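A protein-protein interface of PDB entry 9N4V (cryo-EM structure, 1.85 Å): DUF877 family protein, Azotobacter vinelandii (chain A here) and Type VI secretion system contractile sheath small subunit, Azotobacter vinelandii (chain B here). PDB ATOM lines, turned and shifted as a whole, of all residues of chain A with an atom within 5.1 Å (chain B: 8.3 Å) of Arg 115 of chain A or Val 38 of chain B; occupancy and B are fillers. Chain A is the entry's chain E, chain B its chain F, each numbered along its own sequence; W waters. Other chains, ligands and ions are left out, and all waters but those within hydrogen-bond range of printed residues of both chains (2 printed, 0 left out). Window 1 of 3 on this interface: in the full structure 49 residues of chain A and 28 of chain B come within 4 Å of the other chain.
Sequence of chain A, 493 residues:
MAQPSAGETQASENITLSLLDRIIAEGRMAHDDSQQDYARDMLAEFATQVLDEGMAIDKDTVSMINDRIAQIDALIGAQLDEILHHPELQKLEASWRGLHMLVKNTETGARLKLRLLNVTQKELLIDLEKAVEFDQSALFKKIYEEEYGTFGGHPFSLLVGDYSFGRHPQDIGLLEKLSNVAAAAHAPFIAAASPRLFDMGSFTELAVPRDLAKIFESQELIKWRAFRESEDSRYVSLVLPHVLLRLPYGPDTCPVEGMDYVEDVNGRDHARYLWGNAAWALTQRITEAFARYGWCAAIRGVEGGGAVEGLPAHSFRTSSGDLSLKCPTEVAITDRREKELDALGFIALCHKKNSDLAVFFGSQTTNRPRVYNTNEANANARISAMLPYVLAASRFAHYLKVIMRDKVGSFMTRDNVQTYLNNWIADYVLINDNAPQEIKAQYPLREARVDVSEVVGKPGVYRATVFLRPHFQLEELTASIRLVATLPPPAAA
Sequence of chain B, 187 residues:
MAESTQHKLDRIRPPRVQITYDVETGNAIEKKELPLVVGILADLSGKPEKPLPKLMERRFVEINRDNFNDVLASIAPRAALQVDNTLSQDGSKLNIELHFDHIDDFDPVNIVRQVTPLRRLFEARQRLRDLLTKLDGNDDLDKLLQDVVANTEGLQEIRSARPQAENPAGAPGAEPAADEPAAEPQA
N of Lys 113 of chain A is in hydrogen-bond range of O of Leu 36 of chain B, at 2.8 Å.
The backbone carbonyl oxygen of Lys 113 of chain A sits at hydrogen-bond distance from the backbone NH of Val 38 of chain B, 2.9 Å away.
OE1 of Glu 62 of chain B is in salt-bridge range of NZ of Lys 113 of chain A, at 3.9 Å.
The backbone NH (N) of Ile 63 of chain B lies within hydrogen-bond range of the backbone carbonyl oxygen (O) of Leu 114 of chain A, at 2.8 Å.
The backbone carbonyl oxygen (O) of Val 38 of chain B sits at hydrogen-bond distance from the backbone NH (N) of Arg 115 of chain A, 2.9 Å away.
N of Ile 40 of chain B sits at hydrogen-bond distance from O of Arg 115 of chain A, at 2.8 Å.
NH2 of Arg 115 of chain A lies within hydrogen-bond range of O of Phe 60 of chain B (3.0 Å).
N of Leu 116 of chain A is in hydrogen-bond range of O of Val 61 of chain B.
N of Leu 117 of chain A is in hydrogen-bond range of O of Ile 40 of chain B (2.8 Å).
The backbone carbonyl oxygen of Leu 117 of chain A lies within hydrogen-bond range of the backbone NH of Ala 42 of chain B (3.3 Å).
The backbone NH (N) of Ser 157 of chain A lies within hydrogen-bond range of the backbone carbonyl oxygen (O) of Val 37 of chain B, at 2.7 Å.
N of Leu 158 of chain A sits at hydrogen-bond distance from O of Val 37 of chain B (3.4 Å).
The backbone carbonyl oxygen (O) of Leu 158 of chain A sits at hydrogen-bond distance from the backbone NH (N) of Gly 39 of chain B, at 2.8 Å.
The backbone carbonyl oxygen (O) of Gly 39 of chain B lies within hydrogen-bond range of the backbone NH (N) of Val 160 of chain A (2.9 Å).
O of Val 160 of chain A is in hydrogen-bond range of N of Leu 41 of chain B.
The backbone carbonyl oxygen of Arg 59 of chain B sits close to the backbone carbonyl oxygen of Leu 116 of chain A.
NH1 of Arg 115 of chain A is in salt-bridge range of OE2 of Glu 147 of chain A (3.2 Å).
ND2 of Asn 64 of chain B lies within hydrogen-bond range of OE2 of Glu 62 of chain B (3.1 Å).
Leu 112 of chain A touches Leu 36 of chain B.
CA of Leu 114 of chain A touches O of Val 38 of chain B, 3.6 Å away.
Arg 115 of chain A touches Val 37 of chain B.
O of Arg 115 of chain A touches CA of Gly 39 of chain B (3.5 Å).
Phe 60 of chain B touches Leu 116 of chain A (CA to O, 3.3 Å).
CE1 of Phe 60 of chain B touches CB of Leu 117 of chain A, 3.5 Å away.
C of Phe 156 of chain A touches O of Val 37 of chain B, at 3.6 Å.
Phe 60 of chain B touches Phe 156 of chain A (CG to CZ, 3.7 Å).
Ser 157 of chain A touches Leu 36 of chain B.
Val 160 of chain A touches Ile 40 of chain B.
Arg 115 of chain A touches six residues of chain B.
Of chain A, only Lys 113, Leu 114, Arg 115 and Leu 158 come within 4 Å of Val 38 of chain B.
Of the printed residues of chain B, Leu 158 of chain A touches Val 37 (3.4 Å), Val 38 (3.5 Å) and Gly 39 (2.8 Å).
Printed residues of chain B within 4 Å of Ser 157 of chain A: Pro 35, Leu 36 and Val 37.
Of the printed residues of chain A, Ala 42 of chain B touches Leu 117.
Of the printed residues of chain A, Val 37 of chain B touches Lys 113, Arg 115, Phe 156, Ser 157 and Leu 158.
The nearest printed residue of chain B that does not touch Leu 117 of chain A is Val 61 of chain B (4.9 Å).
Hydrophobic or aromatic side chains of chain A within 4 Å of the printed part of chain B: Leu 114, Leu 116, Leu 117, Phe 156 and Val 160.
Among the printed residues, 35 pairs touch across the chains.
Among the printed residues, Asp or Glu carboxylates within 4 Å of a Lys or Arg side-chain nitrogen of the other chain: Lys 113 of chain A with Glu 62 of chain B.
Water W1 lies within hydrogen-bond range of the backbone carbonyl oxygen of Ile 63 of chain B (2.7 Å), the backbone NH of Leu 114 of chain A (2.8 Å) and the side-chain carboxylate of Glu 62 of chain B (3.1 Å).
Water W2 lies within hydrogen-bond range of the backbone carbonyl oxygen (O) of Arg 59 of chain B (2.8 Å) and the backbone carbonyl oxygen (O) of Leu 116 of chain A (3.2 Å).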
ATOM      1  N   LEU A 112      10.275 -26.068 -16.571  1.00  0.00           N
ATOM      2  CA  LEU A 112      11.692 -25.912 -16.262  1.00  0.00           C
ATOM      3  C   LEU A 112      11.861 -24.834 -15.206  1.00  0.00           C
ATOM      4  O   LEU A 112      11.472 -23.685 -15.430  1.00  0.00           O
ATOM      5  CB  LEU A 112      12.487 -25.552 -17.520  1.00  0.00           C
ATOM      6  CG  LEU A 112      13.923 -26.057 -17.634  1.00  0.00           C
ATOM      7  CD1 LEU A 112      14.433 -25.885 -19.053  1.00  0.00           C
ATOM      8  CD2 LEU A 112      14.824 -25.343 -16.647  1.00  0.00           C
ATOM      9  N   LYS A 113      12.469 -25.193 -14.080  1.00  0.00           N
ATOM     10  CA  LYS A 113      12.657 -24.279 -12.964  1.00  0.00           C
ATOM     11  C   LYS A 113      14.104 -24.304 -12.498  1.00  0.00           C
ATOM     12  O   LYS A 113      14.732 -25.363 -12.441  1.00  0.00           O
ATOM     13  CB  LYS A 113      11.732 -24.637 -11.799  1.00  0.00           C
ATOM     14  CG  LYS A 113      10.396 -23.920 -11.835  1.00  0.00           C
ATOM     15  CD  LYS A 113       9.329 -24.775 -12.479  1.00  0.00           C
ATOM     16  CE  LYS A 113       7.960 -24.112 -12.400  1.00  0.00           C
ATOM     17  NZ  LYS A 113       8.028 -22.642 -12.622  1.00  0.00           N
ATOM     18  N   LEU A 114      14.622 -23.130 -12.160  1.00  0.00           N
ATOM     19  CA  LEU A 114      15.922 -22.981 -11.524  1.00  0.00           C
ATOM     20  C   LEU A 114      15.710 -22.479 -10.104  1.00  0.00           C
ATOM     21  O   LEU A 114      15.025 -21.474  -9.894  1.00  0.00           O
ATOM     22  CB  LEU A 114      16.814 -22.013 -12.301  1.00  0.00           C
ATOM     23  CG  LEU A 114      16.948 -22.251 -13.807  1.00  0.00           C
ATOM     24  CD1 LEU A 114      17.725 -21.125 -14.471  1.00  0.00           C
ATOM     25  CD2 LEU A 114      17.600 -23.594 -14.083  1.00  0.00           C
ATOM     26  N   ARG A 115      16.284 -23.181  -9.135  1.00  0.00           N
ATOM     27  CA  ARG A 115      16.175 -22.825  -7.728  1.00  0.00           C
ATOM     28  C   ARG A 115      17.573 -22.647  -7.158  1.00  0.00           C
ATOM     29  O   ARG A 115      18.453 -23.479  -7.392  1.00  0.00           O
ATOM     30  CB  ARG A 115      15.388 -23.887  -6.955  1.00  0.00           C
ATOM     31  CG  ARG A 115      14.152 -24.369  -7.703  1.00  0.00           C
ATOM     32  CD  ARG A 115      13.157 -25.114  -6.825  1.00  0.00           C
ATOM     33  NE  ARG A 115      13.016 -24.544  -5.492  1.00  0.00           N
ATOM     34  CZ  ARG A 115      12.544 -25.208  -4.447  1.00  0.00           C
ATOM     35  NH1 ARG A 115      12.179 -26.476  -4.540  1.00  0.00           N
ATOM     36  NH2 ARG A 115      12.435 -24.585  -3.278  1.00  0.00           N
ATOM     37  N   LEU A 116      17.775 -21.568  -6.412  1.00  0.00           N
ATOM     38  CA  LEU A 116      19.102 -21.124  -6.013  1.00  0.00           C
ATOM     39  C   LEU A 116      19.229 -21.115  -4.496  1.00  0.00           C
ATOM     40  O   LEU A 116      18.383 -20.544  -3.800  1.00  0.00           O
ATOM     41  CB  LEU A 116      19.386 -19.734  -6.580  1.00  0.00           C
ATOM     42  CG  LEU A 116      20.561 -18.966  -5.985  1.00  0.00           C
ATOM     43  CD1 LEU A 116      21.861 -19.594  -6.434  1.00  0.00           C
ATOM     44  CD2 LEU A 116      20.488 -17.501  -6.380  1.00  0.00           C
ATOM     45  N   LEU A 117      20.292 -21.738  -3.992  1.00  0.00           N
ATOM     46  CA  LEU A 117      20.624 -21.721  -2.574  1.00  0.00           C
ATOM     47  C   LEU A 117      21.960 -21.014  -2.398  1.00  0.00           C
ATOM     48  O   LEU A 117      22.989 -21.503  -2.867  1.00  0.00           O
ATOM     49  CB  LEU A 117      20.687 -23.136  -1.996  1.00  0.00           C
ATOM     50  CG  LEU A 117      21.084 -23.205  -0.518  1.00  0.00           C
ATOM     51  CD1 LEU A 117      19.993 -22.600   0.341  1.00  0.00           C
ATOM     52  CD2 LEU A 117      21.386 -24.633  -0.085  1.00  0.00           C
ATOM     53  N   GLU A 147      11.413 -31.890  -1.266  1.00  0.00           N
ATOM     54  CA  GLU A 147      10.906 -32.061  -2.624  1.00  0.00           C
ATOM     55  C   GLU A 147      10.713 -33.523  -3.002  1.00  0.00           C
ATOM     56  O   GLU A 147       9.585 -33.933  -3.281  1.00  0.00           O
ATOM     57  CB  GLU A 147      11.844 -31.362  -3.615  1.00  0.00           C
ATOM     58  CG  GLU A 147      11.813 -29.839  -3.541  1.00  0.00           C
ATOM     59  CD  GLU A 147      10.404 -29.263  -3.592  1.00  0.00           C
ATOM     60  OE1 GLU A 147       9.569 -29.758  -4.376  1.00  0.00           O
ATOM     61  OE2 GLU A 147      10.133 -28.305  -2.843  1.00  0.00           O
ATOM     62  N   PHE A 156      14.244 -32.357  -7.238  1.00  0.00           N
ATOM     63  CA  PHE A 156      15.391 -31.775  -7.915  1.00  0.00           C
ATOM     64  C   PHE A 156      15.928 -32.752  -8.950  1.00  0.00           C
ATOM     65  O   PHE A 156      16.305 -33.877  -8.617  1.00  0.00           O
ATOM     66  CB  PHE A 156      16.480 -31.428  -6.906  1.00  0.00           C
ATOM     67  CG  PHE A 156      16.225 -30.162  -6.158  1.00  0.00           C
ATOM     68  CD1 PHE A 156      16.428 -28.935  -6.760  1.00  0.00           C
ATOM     69  CD2 PHE A 156      15.780 -30.197  -4.851  1.00  0.00           C
ATOM     70  CE1 PHE A 156      16.200 -27.771  -6.073  1.00  0.00           C
ATOM     71  CE2 PHE A 156      15.551 -29.030  -4.158  1.00  0.00           C
ATOM     72  CZ  PHE A 156      15.760 -27.816  -4.771  1.00  0.00           C
ATOM     73  N   SER A 157      15.952 -32.320 -10.205  1.00  0.00           N
ATOM     74  CA  SER A 157      16.475 -33.165 -11.269  1.00  0.00           C
ATOM     75  C   SER A 157      17.995 -33.209 -11.267  1.00  0.00           C
ATOM     76  O   SER A 157      18.583 -34.244 -11.589  1.00  0.00           O
ATOM     77  CB  SER A 157      15.970 -32.671 -12.624  1.00  0.00           C
ATOM     78  OG  SER A 157      14.593 -32.361 -12.570  1.00  0.00           O
ATOM     79  N   LEU A 158      18.639 -32.105 -10.908  1.00  0.00           N
ATOM     80  CA  LEU A 158      20.081 -31.960 -11.031  1.00  0.00           C
ATOM     81  C   LEU A 158      20.537 -30.890 -10.050  1.00  0.00           C
ATOM     82  O   LEU A 158      19.780 -29.977  -9.721  1.00  0.00           O
ATOM     83  CB  LEU A 158      20.466 -31.585 -12.468  1.00  0.00           C
ATOM     84  CG  LEU A 158      21.763 -30.825 -12.732  1.00  0.00           C
ATOM     85  CD1 LEU A 158      22.924 -31.797 -12.736  1.00  0.00           C
ATOM     86  CD2 LEU A 158      21.692 -30.061 -14.029  1.00  0.00           C
ATOM     87  N   VAL A 160      23.850 -28.212  -9.455  1.00  0.00           N
ATOM     88  CA  VAL A 160      25.087 -27.619  -9.942  1.00  0.00           C
ATOM     89  C   VAL A 160      25.729 -26.856  -8.798  1.00  0.00           C
ATOM     90  O   VAL A 160      25.080 -26.027  -8.151  1.00  0.00           O
ATOM     91  CB  VAL A 160      24.862 -26.710 -11.166  1.00  0.00           C
ATOM     92  CG1 VAL A 160      23.776 -25.684 -10.906  1.00  0.00           C
ATOM     93  CG2 VAL A 160      26.168 -26.035 -11.571  1.00  0.00           C
ATOM     94  N   THR A 283      25.690 -27.149 -17.376  1.00  0.00           N
ATOM     95  CA  THR A 283      24.305 -27.018 -16.942  1.00  0.00           C
ATOM     96  C   THR A 283      23.447 -26.412 -18.041  1.00  0.00           C
ATOM     97  O   THR A 283      22.305 -26.830 -18.250  1.00  0.00           O
ATOM     98  CB  THR A 283      24.225 -26.162 -15.676  1.00  0.00           C
ATOM     99  OG1 THR A 283      25.075 -26.712 -14.665  1.00  0.00           O
ATOM    100  CG2 THR A 283      22.800 -26.109 -15.160  1.00  0.00           C
ATOM    101  N   THR A 287      20.084 -27.940 -19.719  1.00  0.00           N
ATOM    102  CA  THR A 287      18.787 -27.266 -19.757  1.00  0.00           C
ATOM    103  C   THR A 287      18.311 -27.059 -21.190  1.00  0.00           C
ATOM    104  O   THR A 287      17.114 -27.171 -21.468  1.00  0.00           O
ATOM    105  CB  THR A 287      18.833 -25.927 -19.014  1.00  0.00           C
ATOM    106  OG1 THR A 287      19.902 -25.120 -19.518  1.00  0.00           O
ATOM    107  CG2 THR A 287      19.012 -26.144 -17.516  1.00  0.00           C
ATOM    108  N   PRO B  35       8.267 -31.155 -13.911  1.00  0.00           N
ATOM    109  CA  PRO B  35       9.207 -30.175 -14.455  1.00  0.00           C
ATOM    110  C   PRO B  35      10.641 -30.599 -14.186  1.00  0.00           C
ATOM    111  O   PRO B  35      10.927 -31.381 -13.280  1.00  0.00           O
ATOM    112  CB  PRO B  35       8.863 -28.896 -13.691  1.00  0.00           C
ATOM    113  CG  PRO B  35       8.404 -29.400 -12.374  1.00  0.00           C
ATOM    114  CD  PRO B  35       7.656 -30.679 -12.659  1.00  0.00           C
ATOM    115  N   LEU B  36      11.549 -30.077 -15.000  1.00  0.00           N
ATOM    116  CA  LEU B  36      12.967 -30.181 -14.694  1.00  0.00           C
ATOM    117  C   LEU B  36      13.311 -29.118 -13.664  1.00  0.00           C
ATOM    118  O   LEU B  36      13.063 -27.929 -13.888  1.00  0.00           O
ATOM    119  CB  LEU B  36      13.815 -30.006 -15.951  1.00  0.00           C
ATOM    120  CG  LEU B  36      15.317 -30.195 -15.730  1.00  0.00           C
ATOM    121  CD1 LEU B  36      15.700 -31.644 -15.942  1.00  0.00           C
ATOM    122  CD2 LEU B  36      16.123 -29.293 -16.638  1.00  0.00           C
ATOM    123  N   VAL B  37      13.869 -29.535 -12.535  1.00  0.00           N
ATOM    124  CA  VAL B  37      14.225 -28.621 -11.458  1.00  0.00           C
ATOM    125  C   VAL B  37      15.729 -28.699 -11.252  1.00  0.00           C
ATOM    126  O   VAL B  37      16.255 -29.751 -10.871  1.00  0.00           O
ATOM    127  CB  VAL B  37      13.469 -28.944 -10.162  1.00  0.00           C
ATOM    128  CG1 VAL B  37      13.847 -27.962  -9.067  1.00  0.00           C
ATOM    129  CG2 VAL B  37      11.972 -28.926 -10.408  1.00  0.00           C
ATOM    130  N   VAL B  38      16.416 -27.591 -11.492  1.00  0.00           N
ATOM    131  CA  VAL B  38      17.855 -27.500 -11.296  1.00  0.00           C
ATOM    132  C   VAL B  38      18.108 -26.781  -9.981  1.00  0.00           C
ATOM    133  O   VAL B  38      17.698 -25.628  -9.804  1.00  0.00           O
ATOM    134  CB  VAL B  38      18.538 -26.771 -12.464  1.00  0.00           C
ATOM    135  CG1 VAL B  38      20.018 -26.593 -12.187  1.00  0.00           C
ATOM    136  CG2 VAL B  38      18.320 -27.521 -13.771  1.00  0.00           C
ATOM    137  N   GLY B  39      18.772 -27.461  -9.053  1.00  0.00           N
ATOM    138  CA  GLY B  39      19.213 -26.831  -7.827  1.00  0.00           C
ATOM    139  C   GLY B  39      20.608 -26.257  -7.963  1.00  0.00           C
ATOM    140  O   GLY B  39      21.540 -26.972  -8.329  1.00  0.00           O
ATOM    141  N   ILE B  40      20.769 -24.973  -7.673  1.00  0.00           N
ATOM    142  CA  ILE B  40      22.040 -24.278  -7.832  1.00  0.00           C
ATOM    143  C   ILE B  40      22.587 -23.942  -6.452  1.00  0.00           C
ATOM    144  O   ILE B  40      21.887 -23.340  -5.630  1.00  0.00           O
ATOM    145  CB  ILE B  40      21.882 -23.009  -8.687  1.00  0.00           C
ATOM    146  CG1 ILE B  40      21.159 -23.326  -9.998  1.00  0.00           C
ATOM    147  CG2 ILE B  40      23.234 -22.383  -8.965  1.00  0.00           C
ATOM    148  CD1 ILE B  40      20.720 -22.099 -10.764  1.00  0.00           C
ATOM    149  N   LEU B  41      23.828 -24.338  -6.198  1.00  0.00           N
ATOM    150  CA  LEU B  41      24.534 -24.013  -4.962  1.00  0.00           C
ATOM    151  C   LEU B  41      25.677 -23.073  -5.322  1.00  0.00           C
ATOM    152  O   LEU B  41      26.598 -23.462  -6.043  1.00  0.00           O
ATOM    153  CB  LEU B  41      25.062 -25.272  -4.275  1.00  0.00           C
ATOM    154  CG  LEU B  41      24.073 -26.348  -3.835  1.00  0.00           C
ATOM    155  CD1 LEU B  41      24.703 -27.246  -2.788  1.00  0.00           C
ATOM    156  CD2 LEU B  41      22.823 -25.720  -3.293  1.00  0.00           C
ATOM    157  N   ALA B  42      25.615 -21.840  -4.831  1.00  0.00           N
ATOM    158  CA  ALA B  42      26.629 -20.855  -5.176  1.00  0.00           C
ATOM    159  C   ALA B  42      26.848 -19.904  -4.009  1.00  0.00           C
ATOM    160  O   ALA B  42      25.915 -19.564  -3.279  1.00  0.00           O
ATOM    161  CB  ALA B  42      26.247 -20.068  -6.431  1.00  0.00           C
ATOM    162  N   ARG B  59      16.804 -21.036   1.984  1.00  0.00           N
ATOM    163  CA  ARG B  59      15.931 -21.833   1.141  1.00  0.00           C
ATOM    164  C   ARG B  59      16.379 -21.721  -0.308  1.00  0.00           C
ATOM    165  O   ARG B  59      17.143 -20.828  -0.679  1.00  0.00           O
ATOM    166  CB  ARG B  59      14.470 -21.404   1.294  1.00  0.00           C
ATOM    167  CG  ARG B  59      14.182 -19.996   0.820  1.00  0.00           C
ATOM    168  CD  ARG B  59      12.758 -19.586   1.159  1.00  0.00           C
ATOM    169  NE  ARG B  59      12.217 -18.626   0.203  1.00  0.00           N
ATOM    170  CZ  ARG B  59      11.558 -18.955  -0.901  1.00  0.00           C
ATOM    171  NH1 ARG B  59      11.343 -20.219  -1.229  1.00  0.00           N
ATOM    172  NH2 ARG B  59      11.103 -17.992  -1.696  1.00  0.00           N
ATOM    173  N   PHE B  60      15.903 -22.660  -1.118  1.00  0.00           N
ATOM    174  CA  PHE B  60      16.121 -22.638  -2.560  1.00  0.00           C
ATOM    175  C   PHE B  60      15.108 -21.686  -3.176  1.00  0.00           C
ATOM    176  O   PHE B  60      13.944 -22.039  -3.363  1.00  0.00           O
ATOM    177  CB  PHE B  60      15.975 -24.036  -3.146  1.00  0.00           C
ATOM    178  CG  PHE B  60      17.219 -24.866  -3.070  1.00  0.00           C
ATOM    179  CD1 PHE B  60      18.164 -24.816  -4.080  1.00  0.00           C
ATOM    180  CD2 PHE B  60      17.432 -25.721  -2.002  1.00  0.00           C
ATOM    181  CE1 PHE B  60      19.302 -25.593  -4.020  1.00  0.00           C
ATOM    182  CE2 PHE B  60      18.568 -26.497  -1.938  1.00  0.00           C
ATOM    183  CZ  PHE B  60      19.501 -26.435  -2.947  1.00  0.00           C
ATOM    184  N   VAL B  61      15.540 -20.474  -3.497  1.00  0.00           N
ATOM    185  CA  VAL B  61      14.650 -19.466  -4.060  1.00  0.00           C
ATOM    186  C   VAL B  61      14.617 -19.625  -5.575  1.00  0.00           C
ATOM    187  O   VAL B  61      15.663 -19.737  -6.225  1.00  0.00           O
ATOM    188  CB  VAL B  61      15.086 -18.050  -3.645  1.00  0.00           C
ATOM    189  CG1 VAL B  61      15.072 -17.922  -2.125  1.00  0.00           C
ATOM    190  CG2 VAL B  61      16.463 -17.715  -4.177  1.00  0.00           C
ATOM    191  N   GLU B  62      13.415 -19.664  -6.140  1.00  0.00           N
ATOM    192  CA  GLU B  62      13.275 -19.806  -7.582  1.00  0.00           C
ATOM    193  C   GLU B  62      13.769 -18.549  -8.282  1.00  0.00           C
ATOM    194  O   GLU B  62      13.448 -17.430  -7.874  1.00  0.00           O
ATOM    195  CB  GLU B  62      11.822 -20.084  -7.958  1.00  0.00           C
ATOM    196  CG  GLU B  62      11.666 -20.755  -9.310  1.00  0.00           C
ATOM    197  CD  GLU B  62      10.460 -20.256 -10.078  1.00  0.00           C
ATOM    198  OE1 GLU B  62       9.322 -20.524  -9.637  1.00  0.00           O
ATOM    199  OE2 GLU B  62      10.647 -19.600 -11.125  1.00  0.00           O
ATOM    200  N   ILE B  63      14.550 -18.734  -9.341  1.00  0.00           N
ATOM    201  CA  ILE B  63      15.190 -17.631 -10.042  1.00  0.00           C
ATOM    202  C   ILE B  63      14.937 -17.782 -11.536  1.00  0.00           C
ATOM    203  O   ILE B  63      14.927 -18.897 -12.068  1.00  0.00           O
ATOM    204  CB  ILE B  63      16.702 -17.559  -9.729  1.00  0.00           C
ATOM    205  CG1 ILE B  63      17.305 -16.265 -10.276  1.00  0.00           C
ATOM    206  CG2 ILE B  63      17.439 -18.778 -10.267  1.00  0.00           C
ATOM    207  CD1 ILE B  63      18.750 -16.065  -9.912  1.00  0.00           C
ATOM    208  N   ASN B  64      14.704 -16.660 -12.205  1.00  0.00           N
ATOM    209  CA  ASN B  64      14.421 -16.664 -13.629  1.00  0.00           C
ATOM    210  C   ASN B  64      14.814 -15.309 -14.198  1.00  0.00           C
ATOM    211  O   ASN B  64      15.250 -14.414 -13.472  1.00  0.00           O
ATOM    212  CB  ASN B  64      12.950 -16.987 -13.895  1.00  0.00           C
ATOM    213  CG  ASN B  64      12.008 -16.107 -13.100  1.00  0.00           C
ATOM    214  OD1 ASN B  64      12.029 -14.887 -13.224  1.00  0.00           O
ATOM    215  ND2 ASN B  64      11.171 -16.724 -12.283  1.00  0.00           N
HETATM  216  O   HOH W   1      13.129 -20.816 -12.619  1.00  0.00           O
HETATM  217  O   HOH W   2      19.157 -18.975  -1.151  1.00  0.00           O
